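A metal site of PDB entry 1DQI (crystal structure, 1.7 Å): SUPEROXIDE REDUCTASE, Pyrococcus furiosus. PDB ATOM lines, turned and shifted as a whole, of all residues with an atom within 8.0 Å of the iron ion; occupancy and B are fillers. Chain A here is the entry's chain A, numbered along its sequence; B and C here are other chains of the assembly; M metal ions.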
ATOM      1  N   TRP A  11      31.132   0.638 -20.256  1.00  0.00           N
ATOM      2  CA  TRP A  11      32.566   0.862 -20.233  1.00  0.00           C
ATOM      3  C   TRP A  11      32.960   0.222 -21.550  1.00  0.00           C
ATOM      4  O   TRP A  11      32.321  -0.748 -21.975  1.00  0.00           O
ATOM      5  CB  TRP A  11      33.245   0.178 -19.036  1.00  0.00           C
ATOM      6  CG  TRP A  11      33.179  -1.323 -18.988  1.00  0.00           C
ATOM      7  CD1 TRP A  11      33.807  -2.201 -19.820  1.00  0.00           C
ATOM      8  CD2 TRP A  11      32.491  -2.116 -18.015  1.00  0.00           C
ATOM      9  NE1 TRP A  11      33.559  -3.500 -19.424  1.00  0.00           N
ATOM     10  CE2 TRP A  11      32.759  -3.467 -18.316  1.00  0.00           C
ATOM     11  CE3 TRP A  11      31.689  -1.807 -16.904  1.00  0.00           C
ATOM     12  CZ2 TRP A  11      32.237  -4.522 -17.551  1.00  0.00           C
ATOM     13  CZ3 TRP A  11      31.179  -2.854 -16.148  1.00  0.00           C
ATOM     14  CH2 TRP A  11      31.449  -4.188 -16.476  1.00  0.00           C
ATOM     15  N   GLU A  14      32.428  -4.044 -23.267  1.00  0.00           N
ATOM     16  CA  GLU A  14      31.270  -4.897 -23.000  1.00  0.00           C
ATOM     17  C   GLU A  14      29.997  -4.058 -22.940  1.00  0.00           C
ATOM     18  O   GLU A  14      29.937  -3.079 -22.195  1.00  0.00           O
ATOM     19  CB  GLU A  14      31.448  -5.673 -21.696  1.00  0.00           C
ATOM     20  CG  GLU A  14      30.300  -6.625 -21.381  1.00  0.00           C
ATOM     21  CD  GLU A  14      30.661  -7.665 -20.336  1.00  0.00           C
ATOM     22  OE1 GLU A  14      31.842  -8.083 -20.275  1.00  0.00           O
ATOM     23  OE2 GLU A  14      29.767  -8.069 -19.566  1.00  0.00           O
ATOM     24  N   LYS A  15      28.995  -4.446 -23.717  1.00  0.00           N
ATOM     25  CA  LYS A  15      27.727  -3.721 -23.765  1.00  0.00           C
ATOM     26  C   LYS A  15      26.741  -4.236 -22.733  1.00  0.00           C
ATOM     27  O   LYS A  15      26.401  -5.421 -22.720  1.00  0.00           O
ATOM     28  CB  LYS A  15      27.107  -3.846 -25.163  1.00  0.00           C
ATOM     29  CG  LYS A  15      28.000  -3.307 -26.281  1.00  0.00           C
ATOM     30  CD  LYS A  15      27.695  -1.852 -26.571  1.00  0.00           C
ATOM     31  CE  LYS A  15      26.630  -1.711 -27.634  1.00  0.00           C
ATOM     32  NZ  LYS A  15      27.129  -2.130 -28.972  1.00  0.00           N
ATOM     33  N   HIS A  16      26.265  -3.343 -21.869  1.00  0.00           N
ATOM     34  CA  HIS A  16      25.313  -3.690 -20.818  1.00  0.00           C
ATOM     35  C   HIS A  16      24.058  -2.831 -20.866  1.00  0.00           C
ATOM     36  O   HIS A  16      22.969  -3.296 -20.571  1.00  0.00           O
ATOM     37  CB  HIS A  16      25.959  -3.493 -19.445  1.00  0.00           C
ATOM     38  CG  HIS A  16      26.855  -4.608 -19.021  1.00  0.00           C
ATOM     39  ND1 HIS A  16      28.215  -4.471 -18.862  1.00  0.00           N
ATOM     40  CD2 HIS A  16      26.573  -5.900 -18.705  1.00  0.00           C
ATOM     41  CE1 HIS A  16      28.698  -5.660 -18.461  1.00  0.00           C
ATOM     42  NE2 HIS A  16      27.746  -6.554 -18.350  1.00  0.00           N
ATOM     43  N   VAL A  35      20.133  -5.678 -25.122  1.00  0.00           N
ATOM     44  CA  VAL A  35      21.469  -5.493 -24.593  1.00  0.00           C
ATOM     45  C   VAL A  35      22.435  -6.123 -25.607  1.00  0.00           C
ATOM     46  O   VAL A  35      22.262  -7.272 -25.988  1.00  0.00           O
ATOM     47  CB  VAL A  35      21.627  -6.202 -23.231  1.00  0.00           C
ATOM     48  CG1 VAL A  35      23.076  -6.126 -22.770  1.00  0.00           C
ATOM     49  CG2 VAL A  35      20.705  -5.564 -22.205  1.00  0.00           C
ATOM     50  N   HIS A  41      26.634  -9.072 -25.874  1.00  0.00           N
ATOM     51  CA  HIS A  41      27.116  -9.272 -24.520  1.00  0.00           C
ATOM     52  C   HIS A  41      27.257 -10.786 -24.427  1.00  0.00           C
ATOM     53  O   HIS A  41      26.534 -11.529 -25.096  1.00  0.00           O
ATOM     54  CB  HIS A  41      26.066  -8.762 -23.533  1.00  0.00           C
ATOM     55  CG  HIS A  41      26.386  -9.054 -22.096  1.00  0.00           C
ATOM     56  ND1 HIS A  41      26.164 -10.272 -21.486  1.00  0.00           N
ATOM     57  CD2 HIS A  41      26.937  -8.256 -21.145  1.00  0.00           C
ATOM     58  CE1 HIS A  41      26.570 -10.177 -20.216  1.00  0.00           C
ATOM     59  NE2 HIS A  41      27.050  -8.965 -19.957  1.00  0.00           N
ATOM     60  N   PRO A  42      28.206 -11.272 -23.619  1.00  0.00           N
ATOM     61  CA  PRO A  42      28.331 -12.729 -23.522  1.00  0.00           C
ATOM     62  C   PRO A  42      27.037 -13.396 -23.076  1.00  0.00           C
ATOM     63  O   PRO A  42      26.218 -12.786 -22.377  1.00  0.00           O
ATOM     64  CB  PRO A  42      29.451 -12.928 -22.505  1.00  0.00           C
ATOM     65  CG  PRO A  42      30.245 -11.655 -22.555  1.00  0.00           C
ATOM     66  CD  PRO A  42      29.227 -10.583 -22.792  1.00  0.00           C
ATOM     67  N   HIS A  47      28.206 -16.268 -17.501  1.00  0.00           N
ATOM     68  CA  HIS A  47      28.041 -14.826 -17.673  1.00  0.00           C
ATOM     69  C   HIS A  47      26.934 -14.538 -18.679  1.00  0.00           C
ATOM     70  O   HIS A  47      27.059 -14.848 -19.864  1.00  0.00           O
ATOM     71  CB  HIS A  47      29.385 -14.279 -18.158  1.00  0.00           C
ATOM     72  CG  HIS A  47      29.429 -12.793 -18.301  1.00  0.00           C
ATOM     73  ND1 HIS A  47      30.432 -12.114 -18.966  1.00  0.00           N
ATOM     74  CD2 HIS A  47      28.576 -11.838 -17.859  1.00  0.00           C
ATOM     75  CE1 HIS A  47      30.155 -10.810 -18.912  1.00  0.00           C
ATOM     76  NE2 HIS A  47      29.042 -10.579 -18.247  1.00  0.00           N
ATOM     77  N   HIS A  48      25.843 -13.912 -18.230  1.00  0.00           N
ATOM     78  CA  HIS A  48      24.730 -13.638 -19.126  1.00  0.00           C
ATOM     79  C   HIS A  48      23.750 -12.593 -18.600  1.00  0.00           C
ATOM     80  O   HIS A  48      23.737 -12.293 -17.409  1.00  0.00           O
ATOM     81  CB  HIS A  48      23.951 -14.934 -19.359  1.00  0.00           C
ATOM     82  CG  HIS A  48      23.516 -15.591 -18.080  1.00  0.00           C
ATOM     83  ND1 HIS A  48      24.200 -16.649 -17.517  1.00  0.00           N
ATOM     84  CD2 HIS A  48      22.491 -15.307 -17.240  1.00  0.00           C
ATOM     85  CE1 HIS A  48      23.620 -16.980 -16.375  1.00  0.00           C
ATOM     86  NE2 HIS A  48      22.584 -16.183 -16.183  1.00  0.00           N
ATOM     87  N   ILE A  49      22.941 -12.059 -19.501  1.00  0.00           N
ATOM     88  CA  ILE A  49      21.924 -11.077 -19.123  1.00  0.00           C
ATOM     89  C   ILE A  49      20.699 -11.881 -18.669  1.00  0.00           C
ATOM     90  O   ILE A  49      20.185 -12.716 -19.414  1.00  0.00           O
ATOM     91  CB  ILE A  49      21.521 -10.162 -20.309  1.00  0.00           C
ATOM     92  CG1 ILE A  49      22.755  -9.391 -20.812  1.00  0.00           C
ATOM     93  CG2 ILE A  49      20.430  -9.205 -19.874  1.00  0.00           C
ATOM     94  CD1 ILE A  49      23.400  -8.494 -19.756  1.00  0.00           C
ATOM     95  N   TYR A 110      19.690  -6.685 -15.921  1.00  0.00           N
ATOM     96  CA  TYR A 110      20.600  -7.252 -14.947  1.00  0.00           C
ATOM     97  C   TYR A 110      21.545  -8.292 -15.544  1.00  0.00           C
ATOM     98  O   TYR A 110      21.102  -9.240 -16.203  1.00  0.00           O
ATOM     99  CB  TYR A 110      19.780  -7.878 -13.810  1.00  0.00           C
ATOM    100  CG  TYR A 110      20.588  -8.590 -12.734  1.00  0.00           C
ATOM    101  CD1 TYR A 110      21.334  -7.873 -11.795  1.00  0.00           C
ATOM    102  CD2 TYR A 110      20.582  -9.987 -12.653  1.00  0.00           C
ATOM    103  CE1 TYR A 110      22.047  -8.531 -10.798  1.00  0.00           C
ATOM    104  CE2 TYR A 110      21.303 -10.658 -11.649  1.00  0.00           C
ATOM    105  CZ  TYR A 110      22.034  -9.911 -10.733  1.00  0.00           C
ATOM    106  OH  TYR A 110      22.749 -10.554  -9.753  1.00  0.00           O
ATOM    107  N   CYS A 111      22.840  -8.096 -15.330  1.00  0.00           N
ATOM    108  CA  CYS A 111      23.849  -9.046 -15.793  1.00  0.00           C
ATOM    109  C   CYS A 111      24.130  -9.889 -14.547  1.00  0.00           C
ATOM    110  O   CYS A 111      24.275  -9.343 -13.454  1.00  0.00           O
ATOM    111  CB  CYS A 111      25.117  -8.318 -16.244  1.00  0.00           C
ATOM    112  SG  CYS A 111      26.506  -9.426 -16.606  1.00  0.00           S
ATOM    113  N   ASN A 112      24.232 -11.197 -14.702  1.00  0.00           N
ATOM    114  CA  ASN A 112      24.437 -12.035 -13.525  1.00  0.00           C
ATOM    115  C   ASN A 112      25.704 -11.757 -12.716  1.00  0.00           C
ATOM    116  O   ASN A 112      25.769 -12.122 -11.539  1.00  0.00           O
ATOM    117  CB  ASN A 112      24.353 -13.528 -13.896  1.00  0.00           C
ATOM    118  CG  ASN A 112      25.569 -14.020 -14.655  1.00  0.00           C
ATOM    119  OD1 ASN A 112      26.160 -13.295 -15.448  1.00  0.00           O
ATOM    120  ND2 ASN A 112      25.940 -15.280 -14.413  1.00  0.00           N
ATOM    121  N   ILE A 113      26.692 -11.110 -13.317  1.00  0.00           N
ATOM    122  CA  ILE A 113      27.933 -10.783 -12.599  1.00  0.00           C
ATOM    123  C   ILE A 113      28.295  -9.299 -12.644  1.00  0.00           C
ATOM    124  O   ILE A 113      29.245  -8.881 -11.983  1.00  0.00           O
ATOM    125  CB  ILE A 113      29.145 -11.601 -13.136  1.00  0.00           C
ATOM    126  CG1 ILE A 113      29.479 -11.180 -14.562  1.00  0.00           C
ATOM    127  CG2 ILE A 113      28.845 -13.097 -13.063  1.00  0.00           C
ATOM    128  CD1 ILE A 113      30.664 -11.923 -15.164  1.00  0.00           C
ATOM    129  N   HIS A 114      27.538  -8.515 -13.405  1.00  0.00           N
ATOM    130  CA  HIS A 114      27.840  -7.081 -13.534  1.00  0.00           C
ATOM    131  C   HIS A 114      26.747  -6.147 -13.042  1.00  0.00           C
ATOM    132  O   HIS A 114      26.671  -4.980 -13.455  1.00  0.00           O
ATOM    133  CB  HIS A 114      28.177  -6.759 -14.993  1.00  0.00           C
ATOM    134  CG  HIS A 114      29.497  -7.299 -15.436  1.00  0.00           C
ATOM    135  ND1 HIS A 114      29.638  -7.949 -16.639  1.00  0.00           N
ATOM    136  CD2 HIS A 114      30.698  -7.270 -14.808  1.00  0.00           C
ATOM    137  CE1 HIS A 114      30.910  -8.296 -16.717  1.00  0.00           C
ATOM    138  NE2 HIS A 114      31.594  -7.903 -15.637  1.00  0.00           N
ATOM    139  N   GLY A 115      25.898  -6.654 -12.154  1.00  0.00           N
ATOM    140  CA  GLY A 115      24.844  -5.835 -11.577  1.00  0.00           C
ATOM    141  C   GLY A 115      23.753  -5.273 -12.457  1.00  0.00           C
ATOM    142  O   GLY A 115      23.478  -5.761 -13.555  1.00  0.00           O
ATOM    143  N   TRP A 117      21.650  -2.283 -14.664  1.00  0.00           N
ATOM    144  CA  TRP A 117      21.871  -1.276 -15.693  1.00  0.00           C
ATOM    145  C   TRP A 117      20.546  -0.635 -16.090  1.00  0.00           C
ATOM    146  O   TRP A 117      19.491  -1.269 -16.020  1.00  0.00           O
ATOM    147  CB  TRP A 117      22.521  -1.912 -16.910  1.00  0.00           C
ATOM    148  CG  TRP A 117      23.850  -2.471 -16.597  1.00  0.00           C
ATOM    149  CD1 TRP A 117      24.123  -3.654 -15.975  1.00  0.00           C
ATOM    150  CD2 TRP A 117      25.111  -1.837 -16.814  1.00  0.00           C
ATOM    151  NE1 TRP A 117      25.476  -3.795 -15.800  1.00  0.00           N
ATOM    152  CE2 TRP A 117      26.111  -2.693 -16.299  1.00  0.00           C
ATOM    153  CE3 TRP A 117      25.501  -0.619 -17.395  1.00  0.00           C
ATOM    154  CZ2 TRP A 117      27.469  -2.378 -16.356  1.00  0.00           C
ATOM    155  CZ3 TRP A 117      26.859  -0.303 -17.452  1.00  0.00           C
ATOM    156  CH2 TRP A 117      27.822  -1.182 -16.932  1.00  0.00           C
ATOM    157  N   VAL B  79      32.669 -12.136 -11.316  1.00  0.00           N
ATOM    158  CA  VAL B  79      33.685 -11.797 -12.308  1.00  0.00           C
ATOM    159  C   VAL B  79      34.935 -12.637 -12.111  1.00  0.00           C
ATOM    160  O   VAL B  79      35.825 -12.638 -12.956  1.00  0.00           O
ATOM    161  CB  VAL B  79      34.081 -10.301 -12.218  1.00  0.00           C
ATOM    162  CG1 VAL B  79      32.912  -9.434 -12.676  1.00  0.00           C
ATOM    163  CG2 VAL B  79      34.479  -9.956 -10.785  1.00  0.00           C
ATOM    164  N   PHE C  63      29.792  -4.781  -7.922  1.00  0.00           N
ATOM    165  CA  PHE C  63      28.534  -5.198  -8.548  1.00  0.00           C
ATOM    166  C   PHE C  63      27.525  -5.824  -7.603  1.00  0.00           C
ATOM    167  O   PHE C  63      27.819  -6.755  -6.860  1.00  0.00           O
ATOM    168  CB  PHE C  63      28.853  -6.140  -9.709  1.00  0.00           C
ATOM    169  CG  PHE C  63      29.815  -5.566 -10.696  1.00  0.00           C
ATOM    170  CD1 PHE C  63      31.138  -6.006 -10.745  1.00  0.00           C
ATOM    171  CD2 PHE C  63      29.421  -4.547 -11.560  1.00  0.00           C
ATOM    172  CE1 PHE C  63      32.053  -5.440 -11.641  1.00  0.00           C
ATOM    173  CE2 PHE C  63      30.329  -3.970 -12.454  1.00  0.00           C
ATOM    174  CZ  PHE C  63      31.649  -4.422 -12.496  1.00  0.00           C
HETATM  175 FE    FE M   1      28.216  -8.591 -18.169  1.00  0.00          FE
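The side-chain sulfur (SG) of Cys 111 lies close to the backbone NH (N) of Ile 113, at 3.7 Å. The backbone carbonyl oxygen (O) of His 114 sits at hydrogen-bond distance from the indole nitrogen (NE1) of Trp 117 (2.9 Å).
Along chain A the residues within 4 Å of the iron ion span positions 14 to 114.
The iron ion is bound by NE2 of His 16 (2.1 Å), OE2 of Glu 14 (2.2 Å), NE2 of His 47 (2.2 Å), NE2 of His 41 (2.2 Å), ND1 of His 114 (2.2 Å) and SG of Cys 111 (2.5 Å).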
